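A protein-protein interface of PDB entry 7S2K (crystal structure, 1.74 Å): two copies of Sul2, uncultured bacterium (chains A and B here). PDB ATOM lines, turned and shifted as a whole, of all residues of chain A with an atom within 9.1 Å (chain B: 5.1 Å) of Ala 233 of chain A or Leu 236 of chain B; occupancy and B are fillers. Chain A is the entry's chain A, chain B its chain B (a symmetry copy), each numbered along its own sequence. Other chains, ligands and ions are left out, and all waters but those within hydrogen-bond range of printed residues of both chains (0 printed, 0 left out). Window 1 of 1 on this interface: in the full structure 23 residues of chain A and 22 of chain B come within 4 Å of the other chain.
Leu 232 of chain B touches Ala 229 of chain A.
Val 260 of chain B touches Ala 230 of chain A (CG2 to O, 3.7 Å).
Leu 236 of chain B touches Ala 233 of chain A (CD1 to CB, 3.8 Å).
Ala 233 of chain A touches Gly 257 of chain B (CB to CA, 3.5 Å).
Leu 236 of chain A touches Ala 233 of chain B (CD1 to CB, 3.7 Å).
Gly 257 of chain A touches Ala 233 of chain B.
Ala 234 of chain B touches Val 260 of chain A.
Leu 264 of chain A touches Ala 237 of chain B.
Ala 233 of chain A touches just these residues of chain B: Leu 236 (3.8 Å) and Gly 257 (3.5 Å).
Printed residues of chain A within 4 Å of Leu 236 of chain B: Ala 233.
Ala 237 of chain B touches just one residue of chain A: Leu 264.
No residue of chain A comes within 4 Å of Ala 239 of chain B.
Of the printed residues of chain A, Leu 232 of chain B touches Ala 229.
Printed residues of chain B within 4 Å of Ala 230 of chain A: Val 260 (3.7 Å).
Leu 216 of chain A touches none of the printed residues of chain B.
Glu 235 of chain B touches none of the printed residues of chain A.
The nearest residue of chain A that does not touch Leu 236 of chain B is Leu 236 of chain A (4.7 Å).
The nearest printed residue of chain B that does not touch Val 260 of chain A is Ala 233 of chain B (4.1 Å).
Of the 16 printed residues of chain B, 7 touch a printed residue of chain A.
Hydrophobic or aromatic side chains of chain B within 4 Å of the printed part of chain A: Leu 232, Ala 233, Leu 236, Ala 237 and Val 260.
Hydrophobic or aromatic side chains of chain A that line the printed part of chain B: Ala 229, Ala 230, Ala 233, Leu 236, Val 260 and Leu 264.
Among the printed residues, no Asp or Glu carboxylate lies within 4 Å of a Lys or Arg side-chain nitrogen of the other chain.
Ala 233 of chain A touches Leu 236 of chain B, and with the chains exchanged Leu 236 of chain A touches Ala 233 of chain B.
Ala 233 of chain A touches Gly 257 of chain B, and with the chains exchanged Gly 257 of chain A touches Ala 233 of chain B.
Val 260 of chain A touches Ala 234 of chain B, but with the chains exchanged Ala 234 of chain A does not touch Val 260 of chain B (4.05 Å).
Of the 8 pairs that touch across the chains among the printed residues, 4 have their exchanged pair printed and touching as well.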
ATOM      1  N   LEU A 189      22.848 -37.470 -19.643  1.00  0.00           N
ATOM      2  CA  LEU A 189      21.633 -37.085 -20.350  1.00  0.00           C
ATOM      3  C   LEU A 189      20.471 -36.897 -19.382  1.00  0.00           C
ATOM      4  O   LEU A 189      19.635 -36.006 -19.577  1.00  0.00           O
ATOM      5  CB  LEU A 189      21.293 -38.126 -21.420  1.00  0.00           C
ATOM      6  CG  LEU A 189      22.261 -38.157 -22.614  1.00  0.00           C
ATOM      7  CD1 LEU A 189      22.190 -39.492 -23.346  1.00  0.00           C
ATOM      8  CD2 LEU A 189      22.006 -36.996 -23.574  1.00  0.00           C
ATOM      9  N   LEU A 192      21.141 -33.438 -17.816  1.00  0.00           N
ATOM     10  CA  LEU A 192      20.840 -32.382 -18.772  1.00  0.00           C
ATOM     11  C   LEU A 192      19.337 -32.219 -18.967  1.00  0.00           C
ATOM     12  O   LEU A 192      18.855 -31.099 -19.175  1.00  0.00           O
ATOM     13  CB  LEU A 192      21.536 -32.679 -20.101  1.00  0.00           C
ATOM     14  CG  LEU A 192      21.321 -31.691 -21.240  1.00  0.00           C
ATOM     15  CD1 LEU A 192      21.861 -30.327 -20.855  1.00  0.00           C
ATOM     16  CD2 LEU A 192      22.033 -32.219 -22.479  1.00  0.00           C
ATOM     17  N   VAL A 210      28.499 -28.712 -20.381  1.00  0.00           N
ATOM     18  CA  VAL A 210      28.555 -29.888 -21.237  1.00  0.00           C
ATOM     19  C   VAL A 210      29.660 -29.796 -22.282  1.00  0.00           C
ATOM     20  O   VAL A 210      29.962 -30.813 -22.929  1.00  0.00           O
ATOM     21  CB  VAL A 210      27.202 -30.134 -21.941  1.00  0.00           C
ATOM     22  CG1 VAL A 210      26.063 -30.132 -20.928  1.00  0.00           C
ATOM     23  CG2 VAL A 210      26.973 -29.088 -23.024  1.00  0.00           C
ATOM     24  N   PHE A 215      30.669 -37.746 -23.315  1.00  0.00           N
ATOM     25  CA  PHE A 215      29.386 -38.396 -23.562  1.00  0.00           C
ATOM     26  C   PHE A 215      28.761 -37.917 -24.860  1.00  0.00           C
ATOM     27  O   PHE A 215      27.984 -38.658 -25.470  1.00  0.00           O
ATOM     28  CB  PHE A 215      28.402 -38.196 -22.396  1.00  0.00           C
ATOM     29  CG  PHE A 215      27.762 -36.834 -22.341  1.00  0.00           C
ATOM     30  CD1 PHE A 215      28.446 -35.753 -21.807  1.00  0.00           C
ATOM     31  CD2 PHE A 215      26.461 -36.642 -22.799  1.00  0.00           C
ATOM     32  CE1 PHE A 215      27.862 -34.503 -21.749  1.00  0.00           C
ATOM     33  CE2 PHE A 215      25.864 -35.392 -22.741  1.00  0.00           C
ATOM     34  CZ  PHE A 215      26.565 -34.319 -22.218  1.00  0.00           C
ATOM     35  N   LEU A 216      29.114 -36.714 -25.313  1.00  0.00           N
ATOM     36  CA  LEU A 216      28.612 -36.234 -26.595  1.00  0.00           C
ATOM     37  C   LEU A 216      29.235 -36.986 -27.764  1.00  0.00           C
ATOM     38  O   LEU A 216      28.584 -37.167 -28.798  1.00  0.00           O
ATOM     39  CB  LEU A 216      28.874 -34.737 -26.729  1.00  0.00           C
ATOM     40  CG  LEU A 216      28.224 -33.806 -25.710  1.00  0.00           C
ATOM     41  CD1 LEU A 216      28.896 -32.435 -25.767  1.00  0.00           C
ATOM     42  CD2 LEU A 216      26.724 -33.698 -25.949  1.00  0.00           C
ATOM     43  N   LEU A 219      27.341 -40.315 -28.200  1.00  0.00           N
ATOM     44  CA  LEU A 219      26.043 -40.218 -28.856  1.00  0.00           C
ATOM     45  C   LEU A 219      26.156 -39.993 -30.353  1.00  0.00           C
ATOM     46  O   LEU A 219      25.269 -40.412 -31.105  1.00  0.00           O
ATOM     47  CB  LEU A 219      25.204 -39.087 -28.259  1.00  0.00           C
ATOM     48  CG  LEU A 219      25.138 -38.901 -26.753  1.00  0.00           C
ATOM     49  CD1 LEU A 219      24.590 -37.521 -26.413  1.00  0.00           C
ATOM     50  CD2 LEU A 219      24.275 -39.994 -26.166  1.00  0.00           C
ATOM     51  N   THR A 220      27.209 -39.317 -30.806  1.00  0.00           N
ATOM     52  CA  THR A 220      27.338 -38.977 -32.213  1.00  0.00           C
ATOM     53  C   THR A 220      28.270 -39.911 -32.969  1.00  0.00           C
ATOM     54  O   THR A 220      28.271 -39.891 -34.205  1.00  0.00           O
ATOM     55  CB  THR A 220      27.824 -37.531 -32.361  1.00  0.00           C
ATOM     56  OG1 THR A 220      29.081 -37.376 -31.694  1.00  0.00           O
ATOM     57  CG2 THR A 220      26.811 -36.572 -31.739  1.00  0.00           C
ATOM     58  N   VAL A 227      32.987 -32.283 -32.052  1.00  0.00           N
ATOM     59  CA  VAL A 227      31.858 -32.287 -31.134  1.00  0.00           C
ATOM     60  C   VAL A 227      31.265 -30.884 -30.948  1.00  0.00           C
ATOM     61  O   VAL A 227      30.492 -30.648 -30.018  1.00  0.00           O
ATOM     62  CB  VAL A 227      32.267 -32.926 -29.790  1.00  0.00           C
ATOM     63  CG1 VAL A 227      33.143 -31.984 -28.979  1.00  0.00           C
ATOM     64  CG2 VAL A 227      31.056 -33.399 -29.005  1.00  0.00           C
ATOM     65  N   GLY A 228      31.587 -29.952 -31.848  1.00  0.00           N
ATOM     66  CA  GLY A 228      31.018 -28.616 -31.746  1.00  0.00           C
ATOM     67  C   GLY A 228      29.511 -28.597 -31.939  1.00  0.00           C
ATOM     68  O   GLY A 228      28.788 -27.930 -31.192  1.00  0.00           O
ATOM     69  N   ALA A 229      29.015 -29.324 -32.941  1.00  0.00           N
ATOM     70  CA  ALA A 229      27.579 -29.318 -33.205  1.00  0.00           C
ATOM     71  C   ALA A 229      26.807 -29.998 -32.082  1.00  0.00           C
ATOM     72  O   ALA A 229      25.745 -29.514 -31.671  1.00  0.00           O
ATOM     73  CB  ALA A 229      27.286 -29.997 -34.542  1.00  0.00           C
ATOM     74  N   ALA A 230      27.316 -31.129 -31.586  1.00  0.00           N
ATOM     75  CA  ALA A 230      26.652 -31.804 -30.475  1.00  0.00           C
ATOM     76  C   ALA A 230      26.673 -30.940 -29.223  1.00  0.00           C
ATOM     77  O   ALA A 230      25.696 -30.906 -28.465  1.00  0.00           O
ATOM     78  CB  ALA A 230      27.315 -33.156 -30.208  1.00  0.00           C
ATOM     79  N   THR A 231      27.780 -30.228 -28.996  1.00  0.00           N
ATOM     80  CA  THR A 231      27.871 -29.318 -27.860  1.00  0.00           C
ATOM     81  C   THR A 231      26.816 -28.225 -27.940  1.00  0.00           C
ATOM     82  O   THR A 231      26.118 -27.949 -26.956  1.00  0.00           O
ATOM     83  CB  THR A 231      29.269 -28.700 -27.795  1.00  0.00           C
ATOM     84  OG1 THR A 231      30.219 -29.728 -27.505  1.00  0.00           O
ATOM     85  CG2 THR A 231      29.330 -27.626 -26.723  1.00  0.00           C
ATOM     86  N   LEU A 232      26.698 -27.582 -29.102  1.00  0.00           N
ATOM     87  CA  LEU A 232      25.709 -26.523 -29.268  1.00  0.00           C
ATOM     88  C   LEU A 232      24.303 -27.042 -29.014  1.00  0.00           C
ATOM     89  O   LEU A 232      23.510 -26.401 -28.316  1.00  0.00           O
ATOM     90  CB  LEU A 232      25.798 -25.915 -30.667  1.00  0.00           C
ATOM     91  CG  LEU A 232      24.874 -24.709 -30.888  1.00  0.00           C
ATOM     92  CD1 LEU A 232      25.038 -23.648 -29.794  1.00  0.00           C
ATOM     93  CD2 LEU A 232      25.071 -24.107 -32.268  1.00  0.00           C
ATOM     94  N   ALA A 233      23.972 -28.209 -29.578  1.00  0.00           N
ATOM     95  CA  ALA A 233      22.644 -28.778 -29.353  1.00  0.00           C
ATOM     96  C   ALA A 233      22.395 -29.026 -27.871  1.00  0.00           C
ATOM     97  O   ALA A 233      21.309 -28.730 -27.360  1.00  0.00           O
ATOM     98  CB  ALA A 233      22.482 -30.073 -30.146  1.00  0.00           C
ATOM     99  N   ALA A 234      23.389 -29.565 -27.163  1.00  0.00           N
ATOM    100  CA  ALA A 234      23.213 -29.815 -25.736  1.00  0.00           C
ATOM    101  C   ALA A 234      23.102 -28.510 -24.958  1.00  0.00           C
ATOM    102  O   ALA A 234      22.297 -28.405 -24.020  1.00  0.00           O
ATOM    103  CB  ALA A 234      24.363 -30.671 -25.206  1.00  0.00           C
ATOM    104  N   GLU A 235      23.891 -27.501 -25.340  1.00  0.00           N
ATOM    105  CA  GLU A 235      23.843 -26.212 -24.655  1.00  0.00           C
ATOM    106  C   GLU A 235      22.507 -25.515 -24.880  1.00  0.00           C
ATOM    107  O   GLU A 235      21.942 -24.938 -23.947  1.00  0.00           O
ATOM    108  CB  GLU A 235      24.997 -25.322 -25.122  1.00  0.00           C
ATOM    109  CG  GLU A 235      26.265 -25.542 -24.331  1.00  0.00           C
ATOM    110  CD  GLU A 235      27.527 -25.103 -25.043  1.00  0.00           C
ATOM    111  OE1 GLU A 235      27.444 -24.496 -26.137  1.00  0.00           O
ATOM    112  OE2 GLU A 235      28.615 -25.362 -24.484  1.00  0.00           O
ATOM    113  N   LEU A 236      21.983 -25.554 -26.108  1.00  0.00           N
ATOM    114  CA  LEU A 236      20.681 -24.942 -26.346  1.00  0.00           C
ATOM    115  C   LEU A 236      19.561 -25.705 -25.644  1.00  0.00           C
ATOM    116  O   LEU A 236      18.579 -25.094 -25.204  1.00  0.00           O
ATOM    117  CB  LEU A 236      20.401 -24.840 -27.845  1.00  0.00           C
ATOM    118  CG  LEU A 236      21.407 -24.008 -28.644  1.00  0.00           C
ATOM    119  CD1 LEU A 236      21.232 -24.252 -30.134  1.00  0.00           C
ATOM    120  CD2 LEU A 236      21.259 -22.530 -28.313  1.00  0.00           C
ATOM    121  N   ALA A 237      19.677 -27.030 -25.536  1.00  0.00           N
ATOM    122  CA  ALA A 237      18.688 -27.779 -24.767  1.00  0.00           C
ATOM    123  C   ALA A 237      18.751 -27.401 -23.294  1.00  0.00           C
ATOM    124  O   ALA A 237      17.716 -27.320 -22.622  1.00  0.00           O
ATOM    125  CB  ALA A 237      18.897 -29.283 -24.948  1.00  0.00           C
ATOM    126  N   ALA A 238      19.956 -27.146 -22.782  1.00  0.00           N
ATOM    127  CA  ALA A 238      20.095 -26.677 -21.407  1.00  0.00           C
ATOM    128  C   ALA A 238      19.487 -25.291 -21.239  1.00  0.00           C
ATOM    129  O   ALA A 238      18.796 -25.025 -20.250  1.00  0.00           O
ATOM    130  CB  ALA A 238      21.568 -26.673 -21.002  1.00  0.00           C
ATOM    131  N   ALA A 239      19.725 -24.398 -22.203  1.00  0.00           N
ATOM    132  CA  ALA A 239      19.114 -23.075 -22.150  1.00  0.00           C
ATOM    133  C   ALA A 239      17.594 -23.165 -22.171  1.00  0.00           C
ATOM    134  O   ALA A 239      16.912 -22.475 -21.403  1.00  0.00           O
ATOM    135  CB  ALA A 239      19.604 -22.227 -23.316  1.00  0.00           C
ATOM    136  N   ALA A 240      17.046 -24.002 -23.055  1.00  0.00           N
ATOM    137  CA  ALA A 240      15.600 -24.166 -23.128  1.00  0.00           C
ATOM    138  C   ALA A 240      15.048 -24.790 -21.857  1.00  0.00           C
ATOM    139  O   ALA A 240      13.893 -24.532 -21.490  1.00  0.00           O
ATOM    140  CB  ALA A 240      15.230 -25.017 -24.344  1.00  0.00           C
ATOM    141  N   GLY A 241      15.852 -25.609 -21.176  1.00  0.00           N
ATOM    142  CA  GLY A 241      15.476 -26.174 -19.896  1.00  0.00           C
ATOM    143  C   GLY A 241      15.572 -25.223 -18.725  1.00  0.00           C
ATOM    144  O   GLY A 241      15.168 -25.587 -17.614  1.00  0.00           O
ATOM    145  N   ILE A 246      25.861 -21.166 -18.453  1.00  0.00           N
ATOM    146  CA  ILE A 246      26.466 -22.205 -19.274  1.00  0.00           C
ATOM    147  C   ILE A 246      27.955 -21.913 -19.382  1.00  0.00           C
ATOM    148  O   ILE A 246      28.352 -20.799 -19.740  1.00  0.00           O
ATOM    149  CB  ILE A 246      25.823 -22.294 -20.669  1.00  0.00           C
ATOM    150  CG1 ILE A 246      24.351 -22.697 -20.545  1.00  0.00           C
ATOM    151  CG2 ILE A 246      26.571 -23.307 -21.515  1.00  0.00           C
ATOM    152  CD1 ILE A 246      23.684 -23.005 -21.869  1.00  0.00           C
ATOM    153  N   PRO A 253      29.237 -19.544 -31.013  1.00  0.00           N
ATOM    154  CA  PRO A 253      28.115 -20.367 -31.504  1.00  0.00           C
ATOM    155  C   PRO A 253      26.974 -20.427 -30.513  1.00  0.00           C
ATOM    156  O   PRO A 253      25.807 -20.458 -30.916  1.00  0.00           O
ATOM    157  CB  PRO A 253      28.747 -21.752 -31.713  1.00  0.00           C
ATOM    158  CG  PRO A 253      30.220 -21.531 -31.693  1.00  0.00           C
ATOM    159  CD  PRO A 253      30.470 -20.334 -30.859  1.00  0.00           C
ATOM    160  N   LEU A 254      27.288 -20.441 -29.217  1.00  0.00           N
ATOM    161  CA  LEU A 254      26.243 -20.441 -28.200  1.00  0.00           C
ATOM    162  C   LEU A 254      25.456 -19.137 -28.230  1.00  0.00           C
ATOM    163  O   LEU A 254      24.216 -19.149 -28.232  1.00  0.00           O
ATOM    164  CB  LEU A 254      26.865 -20.668 -26.819  1.00  0.00           C
ATOM    165  CG  LEU A 254      25.868 -20.712 -25.661  1.00  0.00           C
ATOM    166  CD1 LEU A 254      24.748 -21.689 -25.963  1.00  0.00           C
ATOM    167  CD2 LEU A 254      26.572 -21.079 -24.354  1.00  0.00           C
ATOM    168  N   GLY A 257      23.191 -19.128 -31.170  1.00  0.00           N
ATOM    169  CA  GLY A 257      22.064 -20.030 -30.983  1.00  0.00           C
ATOM    170  C   GLY A 257      21.051 -19.490 -29.994  1.00  0.00           C
ATOM    171  O   GLY A 257      19.839 -19.630 -30.191  1.00  0.00           O
ATOM    172  N   VAL A 260      18.866 -16.879 -31.621  1.00  0.00           N
ATOM    173  CA  VAL A 260      17.764 -17.454 -32.390  1.00  0.00           C
ATOM    174  C   VAL A 260      16.639 -17.886 -31.459  1.00  0.00           C
ATOM    175  O   VAL A 260      15.466 -17.574 -31.692  1.00  0.00           O
ATOM    176  CB  VAL A 260      18.260 -18.627 -33.256  1.00  0.00           C
ATOM    177  CG1 VAL A 260      17.082 -19.342 -33.913  1.00  0.00           C
ATOM    178  CG2 VAL A 260      19.234 -18.132 -34.315  1.00  0.00           C
ATOM    179  N   LEU A 261      16.978 -18.607 -30.387  1.00  0.00           N
ATOM    180  CA  LEU A 261      15.940 -19.099 -29.486  1.00  0.00           C
ATOM    181  C   LEU A 261      15.221 -17.948 -28.793  1.00  0.00           C
ATOM    182  O   LEU A 261      13.991 -17.963 -28.670  1.00  0.00           O
ATOM    183  CB  LEU A 261      16.538 -20.063 -28.462  1.00  0.00           C
ATOM    184  CG  LEU A 261      17.098 -21.366 -29.037  1.00  0.00           C
ATOM    185  CD1 LEU A 261      17.263 -22.415 -27.943  1.00  0.00           C
ATOM    186  CD2 LEU A 261      16.225 -21.892 -30.172  1.00  0.00           C
ATOM    187  N   LEU A 264      12.915 -16.270 -31.307  1.00  0.00           N
ATOM    188  CA  LEU A 264      11.744 -17.125 -31.471  1.00  0.00           C
ATOM    189  C   LEU A 264      10.776 -16.941 -30.311  1.00  0.00           C
ATOM    190  O   LEU A 264       9.566 -16.789 -30.512  1.00  0.00           O
ATOM    191  CB  LEU A 264      12.182 -18.586 -31.582  1.00  0.00           C
ATOM    192  CG  LEU A 264      12.685 -19.064 -32.942  1.00  0.00           C
ATOM    193  CD1 LEU A 264      12.963 -20.558 -32.911  1.00  0.00           C
ATOM    194  CD2 LEU A 264      11.666 -18.728 -34.026  1.00  0.00           C
ATOM    195  N   THR B 231      22.127 -21.148 -37.992  1.00  0.00           N
ATOM    196  CA  THR B 231      21.413 -22.105 -38.835  1.00  0.00           C
ATOM    197  C   THR B 231      21.074 -23.372 -38.064  1.00  0.00           C
ATOM    198  O   THR B 231      19.935 -23.852 -38.108  1.00  0.00           O
ATOM    199  CB  THR B 231      22.245 -22.448 -40.075  1.00  0.00           C
ATOM    200  OG1 THR B 231      22.322 -21.307 -40.934  1.00  0.00           O
ATOM    201  CG2 THR B 231      21.623 -23.618 -40.844  1.00  0.00           C
ATOM    202  N   LEU B 232      22.059 -23.936 -37.358  1.00  0.00           N
ATOM    203  CA  LEU B 232      21.816 -25.151 -36.585  1.00  0.00           C
ATOM    204  C   LEU B 232      20.733 -24.930 -35.541  1.00  0.00           C
ATOM    205  O   LEU B 232      19.845 -25.770 -35.372  1.00  0.00           O
ATOM    206  CB  LEU B 232      23.102 -25.629 -35.906  1.00  0.00           C
ATOM    207  CG  LEU B 232      23.004 -26.990 -35.195  1.00  0.00           C
ATOM    208  CD1 LEU B 232      22.414 -28.059 -36.114  1.00  0.00           C
ATOM    209  CD2 LEU B 232      24.353 -27.438 -34.609  1.00  0.00           C
ATOM    210  N   ALA B 233      20.805 -23.810 -34.814  1.00  0.00           N
ATOM    211  CA  ALA B 233      19.806 -23.526 -33.788  1.00  0.00           C
ATOM    212  C   ALA B 233      18.410 -23.464 -34.389  1.00  0.00           C
ATOM    213  O   ALA B 233      17.459 -24.035 -33.842  1.00  0.00           O
ATOM    214  CB  ALA B 233      20.141 -22.216 -33.075  1.00  0.00           C
ATOM    215  N   ALA B 234      18.269 -22.772 -35.522  1.00  0.00           N
ATOM    216  CA  ALA B 234      16.968 -22.670 -36.176  1.00  0.00           C
ATOM    217  C   ALA B 234      16.497 -24.024 -36.690  1.00  0.00           C
ATOM    218  O   ALA B 234      15.305 -24.348 -36.603  1.00  0.00           O
ATOM    219  CB  ALA B 234      17.036 -21.659 -37.319  1.00  0.00           C
ATOM    220  N   GLU B 235      17.414 -24.826 -37.234  1.00  0.00           N
ATOM    221  CA  GLU B 235      17.044 -26.142 -37.748  1.00  0.00           C
ATOM    222  C   GLU B 235      16.614 -27.077 -36.625  1.00  0.00           C
ATOM    223  O   GLU B 235      15.646 -27.835 -36.774  1.00  0.00           O
ATOM    224  CB  GLU B 235      18.210 -26.739 -38.532  1.00  0.00           C
ATOM    225  CG  GLU B 235      18.316 -26.151 -39.922  1.00  0.00           C
ATOM    226  CD  GLU B 235      19.620 -26.471 -40.616  1.00  0.00           C
ATOM    227  OE1 GLU B 235      20.550 -26.990 -39.960  1.00  0.00           O
ATOM    228  OE2 GLU B 235      19.705 -26.192 -41.833  1.00  0.00           O
ATOM    229  N   LEU B 236      17.323 -27.050 -35.496  1.00  0.00           N
ATOM    230  CA  LEU B 236      16.911 -27.873 -34.362  1.00  0.00           C
ATOM    231  C   LEU B 236      15.572 -27.419 -33.795  1.00  0.00           C
ATOM    232  O   LEU B 236      14.754 -28.252 -33.384  1.00  0.00           O
ATOM    233  CB  LEU B 236      17.987 -27.856 -33.277  1.00  0.00           C
ATOM    234  CG  LEU B 236      19.333 -28.461 -33.672  1.00  0.00           C
ATOM    235  CD1 LEU B 236      20.411 -28.125 -32.626  1.00  0.00           C
ATOM    236  CD2 LEU B 236      19.206 -29.965 -33.855  1.00  0.00           C
ATOM    237  N   ALA B 237      15.332 -26.106 -33.745  1.00  0.00           N
ATOM    238  CA  ALA B 237      14.025 -25.626 -33.305  1.00  0.00           C
ATOM    239  C   ALA B 237      12.926 -26.136 -34.225  1.00  0.00           C
ATOM    240  O   ALA B 237      11.850 -26.534 -33.759  1.00  0.00           O
ATOM    241  CB  ALA B 237      14.008 -24.097 -33.247  1.00  0.00           C
ATOM    242  N   ALA B 238      13.191 -26.156 -35.533  1.00  0.00           N
ATOM    243  CA  ALA B 238      12.199 -26.637 -36.494  1.00  0.00           C
ATOM    244  C   ALA B 238      11.966 -28.134 -36.347  1.00  0.00           C
ATOM    245  O   ALA B 238      10.821 -28.595 -36.384  1.00  0.00           O
ATOM    246  CB  ALA B 238      12.642 -26.304 -37.918  1.00  0.00           C
ATOM    247  N   ALA B 239      13.044 -28.906 -36.187  1.00  0.00           N
ATOM    248  CA  ALA B 239      12.900 -30.335 -35.933  1.00  0.00           C
ATOM    249  C   ALA B 239      12.096 -30.580 -34.666  1.00  0.00           C
ATOM    250  O   ALA B 239      11.143 -31.370 -34.660  1.00  0.00           O
ATOM    251  CB  ALA B 239      14.275 -30.987 -35.824  1.00  0.00           C
ATOM    252  N   ALA B 240      12.466 -29.898 -33.578  1.00  0.00           N
ATOM    253  CA  ALA B 240      11.733 -30.035 -32.324  1.00  0.00           C
ATOM    254  C   ALA B 240      10.284 -29.594 -32.468  1.00  0.00           C
ATOM    255  O   ALA B 240       9.405 -30.112 -31.770  1.00  0.00           O
ATOM    256  CB  ALA B 240      12.424 -29.230 -31.222  1.00  0.00           C
ATOM    257  N   GLY B 241      10.016 -28.641 -33.356  1.00  0.00           N
ATOM    258  CA  GLY B 241       8.676 -28.161 -33.612  1.00  0.00           C
ATOM    259  C   GLY B 241       7.872 -28.961 -34.609  1.00  0.00           C
ATOM    260  O   GLY B 241       6.738 -28.580 -34.919  1.00  0.00           O
ATOM    261  N   LEU B 254      23.532 -30.941 -38.353  1.00  0.00           N
ATOM    262  CA  LEU B 254      22.127 -31.175 -38.034  1.00  0.00           C
ATOM    263  C   LEU B 254      21.920 -32.589 -37.508  1.00  0.00           C
ATOM    264  O   LEU B 254      21.293 -32.786 -36.459  1.00  0.00           O
ATOM    265  CB  LEU B 254      21.261 -30.910 -39.268  1.00  0.00           C
ATOM    266  CG  LEU B 254      19.741 -31.045 -39.150  1.00  0.00           C
ATOM    267  CD1 LEU B 254      19.198 -30.295 -37.947  1.00  0.00           C
ATOM    268  CD2 LEU B 254      19.090 -30.533 -40.433  1.00  0.00           C
ATOM    269  N   GLY B 257      23.247 -32.710 -33.997  1.00  0.00           N
ATOM    270  CA  GLY B 257      22.326 -32.093 -33.058  1.00  0.00           C
ATOM    271  C   GLY B 257      21.090 -32.936 -32.826  1.00  0.00           C
ATOM    272  O   GLY B 257      20.633 -33.091 -31.689  1.00  0.00           O
ATOM    273  N   LEU B 258      20.541 -33.510 -33.900  1.00  0.00           N
ATOM    274  CA  LEU B 258      19.374 -34.377 -33.765  1.00  0.00           C
ATOM    275  C   LEU B 258      19.694 -35.617 -32.939  1.00  0.00           C
ATOM    276  O   LEU B 258      18.829 -36.117 -32.209  1.00  0.00           O
ATOM    277  CB  LEU B 258      18.866 -34.768 -35.152  1.00  0.00           C
ATOM    278  CG  LEU B 258      18.312 -33.603 -35.973  1.00  0.00           C
ATOM    279  CD1 LEU B 258      17.969 -34.087 -37.353  1.00  0.00           C
ATOM    280  CD2 LEU B 258      17.109 -32.971 -35.291  1.00  0.00           C
ATOM    281  N   VAL B 260      21.691 -35.686 -30.361  1.00  0.00           N
ATOM    282  CA  VAL B 260      21.606 -35.257 -28.965  1.00  0.00           C
ATOM    283  C   VAL B 260      20.152 -35.199 -28.518  1.00  0.00           C
ATOM    284  O   VAL B 260      19.791 -35.683 -27.439  1.00  0.00           O
ATOM    285  CB  VAL B 260      22.302 -33.899 -28.771  1.00  0.00           C
ATOM    286  CG1 VAL B 260      22.079 -33.388 -27.343  1.00  0.00           C
ATOM    287  CG2 VAL B 260      23.786 -34.018 -29.062  1.00  0.00           C
ATOM    288  N   LEU B 261      19.294 -34.598 -29.342  1.00  0.00           N
ATOM    289  CA  LEU B 261      17.889 -34.481 -28.972  1.00  0.00           C
ATOM    290  C   LEU B 261      17.227 -35.850 -28.894  1.00  0.00           C
ATOM    291  O   LEU B 261      16.456 -36.119 -27.965  1.00  0.00           O
ATOM    292  CB  LEU B 261      17.171 -33.567 -29.964  1.00  0.00           C
ATOM    293  CG  LEU B 261      17.792 -32.167 -30.002  1.00  0.00           C
ATOM    294  CD1 LEU B 261      16.898 -31.188 -30.745  1.00  0.00           C
ATOM    295  CD2 LEU B 261      18.091 -31.667 -28.586  1.00  0.00           C
